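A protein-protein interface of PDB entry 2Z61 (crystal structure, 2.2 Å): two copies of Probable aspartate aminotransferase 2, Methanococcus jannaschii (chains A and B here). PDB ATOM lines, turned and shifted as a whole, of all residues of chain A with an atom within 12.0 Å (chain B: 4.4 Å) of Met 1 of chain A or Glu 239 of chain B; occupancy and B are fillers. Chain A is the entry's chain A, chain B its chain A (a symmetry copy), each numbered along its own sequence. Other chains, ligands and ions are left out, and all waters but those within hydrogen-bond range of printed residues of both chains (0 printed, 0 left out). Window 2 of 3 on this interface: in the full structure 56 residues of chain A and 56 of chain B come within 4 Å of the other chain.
No position is printed for both chains.
Of the 5 pairs that touch across the chains among the printed residues, none has its exchanged pair printed and touching as well.
Tyr 185 of chain B touches Met 1 of chain A.
CB of Ala 243 of chain B touches CD2 of Leu 2 of chain A, at 3.98 Å.
Ser 3 of chain A touches Ile 109 of chain B.
Leu 6 of chain A touches Ala 243 of chain B.
The side-chain sulfur (SD) of Met 1 of chain A lies close to the side-chain carboxylate (OE1) of Glu 239 of chain B, 3.2 Å away.
Hydrophobic or aromatic side chains of chain B that line the printed part of chain A: Tyr 185 and Ala 243.
Of the 10 printed residues of chain A, 4 touch a printed residue of chain B.
Printed residues of chain A that touch a printed residue of chain B: Met 1, Leu 2, Ser 3 and Leu 6.
Along chain A the printed residues that touch a printed residue of chain B span positions 1 to 6.
Among the printed residues, no Asp or Glu carboxylate lies within 4 Å of a Lys or Arg side-chain nitrogen of the other chain.
The side-chain hydroxyl (OG) of Ser 3 of chain A sits at hydrogen-bond distance from the backbone NH (N) of Leu 6 of chain A.
N of Glu 239 of chain B is in hydrogen-bond range of OD1 of Asn 237 of chain B (3.1 Å).
Met 1 of chain A touches just these residues of chain B: Tyr 185 and Glu 239.
Of chain A, only Met 1 (3.2 Å) comes within 4 Å of Glu 239 of chain B.
Of the printed residues of chain A, Ile 109 of chain B touches Ser 3 (3.7 Å).
No residue of chain A comes within 4 Å of Ile 240 of chain B.
No residue of chain A comes within 4 Å of Ile 241 of chain B.
Glu 242 of chain B touches none of the printed residues of chain A.
Of the printed residues of chain A, Tyr 185 of chain B touches Met 1 (3.1 Å).
Of the printed residues of chain B, Leu 6 of chain A touches Ala 243.
Printed residues of chain B within 4 Å of Leu 2 of chain A: Ala 243 (3.98 Å).
Of the printed residues of chain A, Ala 243 of chain B touches Leu 2 and Leu 6.
Of the printed residues of chain B, Ser 3 of chain A touches Ile 109 (3.7 Å).
Arg 5 of chain A touches none of the printed residues of chain B.
Asn 8 of chain A touches none of the printed residues of chain B.
The nearest residue of chain B that does not touch Met 1 of chain A is Ile 109 of chain B (4.3 Å).
The nearest residue of chain A that does not touch Glu 239 of chain B is Leu 2 of chain A (4.1 Å).
The nearest printed residue of chain A that does not touch Ala 243 of chain B is Phe 9 of chain A (6.3 Å).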
ATOM      1  N   MET A   1      -0.567 -22.644 -12.162  1.00  0.00           N
ATOM      2  CA  MET A   1      -0.304 -22.471 -10.706  1.00  0.00           C
ATOM      3  C   MET A   1      -0.489 -21.024 -10.247  1.00  0.00           C
ATOM      4  O   MET A   1      -1.119 -20.769  -9.218  1.00  0.00           O
ATOM      5  CB  MET A   1       1.109 -22.970 -10.366  1.00  0.00           C
ATOM      6  CG  MET A   1       2.148 -22.726 -11.452  1.00  0.00           C
ATOM      7  SD  MET A   1       3.782 -23.397 -11.029  1.00  0.00           S
ATOM      8  CE  MET A   1       3.475 -25.173 -11.113  1.00  0.00           C
ATOM      9  N   LEU A   2       0.047 -20.079 -11.015  1.00  0.00           N
ATOM     10  CA  LEU A   2      -0.085 -18.663 -10.682  1.00  0.00           C
ATOM     11  C   LEU A   2      -1.539 -18.227 -10.840  1.00  0.00           C
ATOM     12  O   LEU A   2      -2.288 -18.806 -11.627  1.00  0.00           O
ATOM     13  CB  LEU A   2       0.799 -17.810 -11.594  1.00  0.00           C
ATOM     14  CG  LEU A   2       2.314 -17.862 -11.388  1.00  0.00           C
ATOM     15  CD1 LEU A   2       2.985 -16.950 -12.403  1.00  0.00           C
ATOM     16  CD2 LEU A   2       2.665 -17.426  -9.974  1.00  0.00           C
ATOM     17  N   SER A   3      -1.939 -17.201 -10.098  1.00  0.00           N
ATOM     18  CA  SER A   3      -3.311 -16.710 -10.177  1.00  0.00           C
ATOM     19  C   SER A   3      -3.594 -16.049 -11.522  1.00  0.00           C
ATOM     20  O   SER A   3      -2.675 -15.662 -12.241  1.00  0.00           O
ATOM     21  CB  SER A   3      -3.568 -15.692  -9.073  1.00  0.00           C
ATOM     22  OG  SER A   3      -2.783 -14.536  -9.291  1.00  0.00           O
ATOM     23  N   LYS A   4      -4.875 -15.921 -11.848  1.00  0.00           N
ATOM     24  CA  LYS A   4      -5.298 -15.293 -13.092  1.00  0.00           C
ATOM     25  C   LYS A   4      -4.870 -13.829 -13.144  1.00  0.00           C
ATOM     26  O   LYS A   4      -4.438 -13.344 -14.186  1.00  0.00           O
ATOM     27  CB  LYS A   4      -6.821 -15.370 -13.244  1.00  0.00           C
ATOM     28  CG  LYS A   4      -7.364 -16.739 -13.626  1.00  0.00           C
ATOM     29  CD  LYS A   4      -8.849 -16.638 -13.972  1.00  0.00           C
ATOM     30  CE  LYS A   4      -9.422 -17.967 -14.448  1.00  0.00           C
ATOM     31  NZ  LYS A   4     -10.878 -17.854 -14.769  1.00  0.00           N
ATOM     32  N   ARG A   5      -4.998 -13.125 -12.022  1.00  0.00           N
ATOM     33  CA  ARG A   5      -4.621 -11.713 -11.970  1.00  0.00           C
ATOM     34  C   ARG A   5      -3.184 -11.472 -12.406  1.00  0.00           C
ATOM     35  O   ARG A   5      -2.920 -10.612 -13.241  1.00  0.00           O
ATOM     36  CB  ARG A   5      -4.796 -11.147 -10.559  1.00  0.00           C
ATOM     37  CG  ARG A   5      -6.228 -11.039 -10.091  1.00  0.00           C
ATOM     38  CD  ARG A   5      -6.326 -10.139  -8.873  1.00  0.00           C
ATOM     39  NE  ARG A   5      -7.711  -9.977  -8.448  1.00  0.00           N
ATOM     40  CZ  ARG A   5      -8.390 -10.873  -7.740  1.00  0.00           C
ATOM     41  NH1 ARG A   5      -7.808 -12.003  -7.363  1.00  0.00           N
ATOM     42  NH2 ARG A   5      -9.659 -10.644  -7.426  1.00  0.00           N
ATOM     43  N   LEU A   6      -2.255 -12.225 -11.831  1.00  0.00           N
ATOM     44  CA  LEU A   6      -0.845 -12.067 -12.157  1.00  0.00           C
ATOM     45  C   LEU A   6      -0.530 -12.437 -13.592  1.00  0.00           C
ATOM     46  O   LEU A   6       0.505 -12.042 -14.129  1.00  0.00           O
ATOM     47  CB  LEU A   6       0.014 -12.904 -11.208  1.00  0.00           C
ATOM     48  CG  LEU A   6       0.660 -12.133 -10.054  1.00  0.00           C
ATOM     49  CD1 LEU A   6       1.802 -11.290 -10.592  1.00  0.00           C
ATOM     50  CD2 LEU A   6      -0.380 -11.256  -9.367  1.00  0.00           C
ATOM     51  N   LEU A   7      -1.430 -13.193 -14.211  1.00  0.00           N
ATOM     52  CA  LEU A   7      -1.247 -13.628 -15.588  1.00  0.00           C
ATOM     53  C   LEU A   7      -1.564 -12.512 -16.576  1.00  0.00           C
ATOM     54  O   LEU A   7      -1.071 -12.516 -17.703  1.00  0.00           O
ATOM     55  CB  LEU A   7      -2.129 -14.850 -15.865  1.00  0.00           C
ATOM     56  CG  LEU A   7      -1.829 -16.090 -15.009  1.00  0.00           C
ATOM     57  CD1 LEU A   7      -2.875 -17.161 -15.280  1.00  0.00           C
ATOM     58  CD2 LEU A   7      -0.428 -16.615 -15.308  1.00  0.00           C
ATOM     59  N   ASN A   8      -2.377 -11.553 -16.147  1.00  0.00           N
ATOM     60  CA  ASN A   8      -2.751 -10.431 -17.002  1.00  0.00           C
ATOM     61  C   ASN A   8      -1.841  -9.226 -16.781  1.00  0.00           C
ATOM     62  O   ASN A   8      -1.848  -8.284 -17.569  1.00  0.00           O
ATOM     63  CB  ASN A   8      -4.204 -10.026 -16.740  1.00  0.00           C
ATOM     64  CG  ASN A   8      -5.188 -11.140 -17.060  1.00  0.00           C
ATOM     65  OD1 ASN A   8      -5.256 -11.618 -18.195  1.00  0.00           O
ATOM     66  ND2 ASN A   8      -5.961 -11.553 -16.059  1.00  0.00           N
ATOM     67  N   PHE A   9      -1.062  -9.267 -15.704  1.00  0.00           N
ATOM     68  CA  PHE A   9      -0.145  -8.183 -15.349  1.00  0.00           C
ATOM     69  C   PHE A   9       0.942  -7.988 -16.408  1.00  0.00           C
ATOM     70  O   PHE A   9       1.935  -8.717 -16.424  1.00  0.00           O
ATOM     71  CB  PHE A   9       0.523  -8.498 -14.009  1.00  0.00           C
ATOM     72  CG  PHE A   9       0.427  -7.392 -13.006  1.00  0.00           C
ATOM     73  CD1 PHE A   9      -0.756  -7.166 -12.318  1.00  0.00           C
ATOM     74  CD2 PHE A   9       1.523  -6.582 -12.741  1.00  0.00           C
ATOM     75  CE1 PHE A   9      -0.846  -6.148 -11.375  1.00  0.00           C
ATOM     76  CE2 PHE A   9       1.442  -5.564 -11.801  1.00  0.00           C
ATOM     77  CZ  PHE A   9       0.254  -5.347 -11.118  1.00  0.00           C
ATOM     78  N   SER A  11       4.137  -6.442 -18.531  1.00  0.00           N
ATOM     79  CA  SER A  11       5.466  -6.000 -18.119  1.00  0.00           C
ATOM     80  C   SER A  11       5.871  -4.717 -18.836  1.00  0.00           C
ATOM     81  O   SER A  11       5.375  -4.418 -19.920  1.00  0.00           O
ATOM     82  CB  SER A  11       6.498  -7.090 -18.415  1.00  0.00           C
ATOM     83  OG  SER A  11       6.261  -8.244 -17.630  1.00  0.00           O
ATOM     84  N   ILE B 109      -1.139 -16.190  -6.111  1.00  0.00           N
ATOM     85  CA  ILE B 109      -1.626 -17.560  -6.255  1.00  0.00           C
ATOM     86  C   ILE B 109      -3.121 -17.783  -6.022  1.00  0.00           C
ATOM     87  O   ILE B 109      -3.613 -18.889  -6.219  1.00  0.00           O
ATOM     88  CB  ILE B 109      -0.850 -18.518  -5.300  1.00  0.00           C
ATOM     89  CG1 ILE B 109      -1.313 -18.312  -3.852  1.00  0.00           C
ATOM     90  CG2 ILE B 109       0.647 -18.251  -5.388  1.00  0.00           C
ATOM     91  CD1 ILE B 109      -0.492 -19.088  -2.826  1.00  0.00           C
ATOM     92  N   TYR B 185      -0.547 -25.017  -1.510  1.00  0.00           N
ATOM     93  CA  TYR B 185       0.364 -23.945  -1.114  1.00  0.00           C
ATOM     94  C   TYR B 185       0.389 -23.671   0.383  1.00  0.00           C
ATOM     95  O   TYR B 185      -0.651 -23.604   1.027  1.00  0.00           O
ATOM     96  CB  TYR B 185       0.029 -22.634  -1.843  1.00  0.00           C
ATOM     97  CG  TYR B 185       0.436 -22.620  -3.289  1.00  0.00           C
ATOM     98  CD1 TYR B 185      -0.518 -22.707  -4.299  1.00  0.00           C
ATOM     99  CD2 TYR B 185       1.778 -22.561  -3.651  1.00  0.00           C
ATOM    100  CE1 TYR B 185      -0.143 -22.737  -5.637  1.00  0.00           C
ATOM    101  CE2 TYR B 185       2.163 -22.591  -4.985  1.00  0.00           C
ATOM    102  CZ  TYR B 185       1.197 -22.681  -5.971  1.00  0.00           C
ATOM    103  OH  TYR B 185       1.566 -22.729  -7.290  1.00  0.00           O
ATOM    104  N   ASN B 237      10.063 -19.897  -4.428  1.00  0.00           N
ATOM    105  CA  ASN B 237      10.734 -20.347  -5.649  1.00  0.00           C
ATOM    106  C   ASN B 237      10.698 -19.258  -6.727  1.00  0.00           C
ATOM    107  O   ASN B 237       9.983 -18.263  -6.599  1.00  0.00           O
ATOM    108  CB  ASN B 237      10.096 -21.645  -6.174  1.00  0.00           C
ATOM    109  CG  ASN B 237       8.646 -21.464  -6.588  1.00  0.00           C
ATOM    110  OD1 ASN B 237       8.340 -20.708  -7.509  1.00  0.00           O
ATOM    111  ND2 ASN B 237       7.745 -22.161  -5.903  1.00  0.00           N
ATOM    112  N   ASP B 238      11.471 -19.463  -7.790  1.00  0.00           N
ATOM    113  CA  ASP B 238      11.584 -18.509  -8.892  1.00  0.00           C
ATOM    114  C   ASP B 238      10.277 -17.981  -9.467  1.00  0.00           C
ATOM    115  O   ASP B 238      10.100 -16.769  -9.586  1.00  0.00           O
ATOM    116  CB  ASP B 238      12.406 -19.119 -10.031  1.00  0.00           C
ATOM    117  CG  ASP B 238      13.834 -19.428  -9.624  1.00  0.00           C
ATOM    118  OD1 ASP B 238      14.558 -18.503  -9.192  1.00  0.00           O
ATOM    119  OD2 ASP B 238      14.233 -20.606  -9.736  1.00  0.00           O
ATOM    120  N   GLU B 239       9.369 -18.881  -9.837  1.00  0.00           N
ATOM    121  CA  GLU B 239       8.096 -18.468 -10.424  1.00  0.00           C
ATOM    122  C   GLU B 239       7.282 -17.547  -9.529  1.00  0.00           C
ATOM    123  O   GLU B 239       6.707 -16.570  -9.998  1.00  0.00           O
ATOM    124  CB  GLU B 239       7.252 -19.685 -10.800  1.00  0.00           C
ATOM    125  CG  GLU B 239       7.845 -20.506 -11.934  1.00  0.00           C
ATOM    126  CD  GLU B 239       6.964 -21.676 -12.335  1.00  0.00           C
ATOM    127  OE1 GLU B 239       5.771 -21.446 -12.633  1.00  0.00           O
ATOM    128  OE2 GLU B 239       7.464 -22.822 -12.355  1.00  0.00           O
ATOM    129  N   ILE B 240       7.226 -17.863  -8.241  1.00  0.00           N
ATOM    130  CA  ILE B 240       6.475 -17.044  -7.310  1.00  0.00           C
ATOM    131  C   ILE B 240       7.178 -15.714  -7.032  1.00  0.00           C
ATOM    132  O   ILE B 240       6.532 -14.662  -6.983  1.00  0.00           O
ATOM    133  CB  ILE B 240       6.218 -17.815  -6.002  1.00  0.00           C
ATOM    134  CG1 ILE B 240       5.161 -18.892  -6.261  1.00  0.00           C
ATOM    135  CG2 ILE B 240       5.767 -16.864  -4.905  1.00  0.00           C
ATOM    136  CD1 ILE B 240       4.719 -19.632  -5.030  1.00  0.00           C
ATOM    137  N   ILE B 241       8.497 -15.751  -6.873  1.00  0.00           N
ATOM    138  CA  ILE B 241       9.251 -14.533  -6.609  1.00  0.00           C
ATOM    139  C   ILE B 241       9.162 -13.576  -7.789  1.00  0.00           C
ATOM    140  O   ILE B 241       9.038 -12.367  -7.607  1.00  0.00           O
ATOM    141  CB  ILE B 241      10.739 -14.837  -6.314  1.00  0.00           C
ATOM    142  CG1 ILE B 241      10.880 -15.440  -4.918  1.00  0.00           C
ATOM    143  CG2 ILE B 241      11.565 -13.569  -6.412  1.00  0.00           C
ATOM    144  CD1 ILE B 241      10.390 -14.533  -3.789  1.00  0.00           C
ATOM    145  N   GLU B 242       9.211 -14.121  -9.000  1.00  0.00           N
ATOM    146  CA  GLU B 242       9.129 -13.312 -10.207  1.00  0.00           C
ATOM    147  C   GLU B 242       7.772 -12.610 -10.279  1.00  0.00           C
ATOM    148  O   GLU B 242       7.668 -11.474 -10.748  1.00  0.00           O
ATOM    149  CB  GLU B 242       9.313 -14.201 -11.438  1.00  0.00           C
ATOM    150  CG  GLU B 242      10.104 -13.555 -12.563  1.00  0.00           C
ATOM    151  CD  GLU B 242      11.530 -13.209 -12.151  1.00  0.00           C
ATOM    152  OE1 GLU B 242      12.266 -14.126 -11.718  1.00  0.00           O
ATOM    153  OE2 GLU B 242      11.916 -12.022 -12.264  1.00  0.00           O
ATOM    154  N   ALA B 243       6.732 -13.298  -9.814  1.00  0.00           N
ATOM    155  CA  ALA B 243       5.387 -12.749  -9.832  1.00  0.00           C
ATOM    156  C   ALA B 243       5.244 -11.629  -8.801  1.00  0.00           C
ATOM    157  O   ALA B 243       4.643 -10.592  -9.076  1.00  0.00           O
ATOM    158  CB  ALA B 243       4.370 -13.852  -9.556  1.00  0.00           C
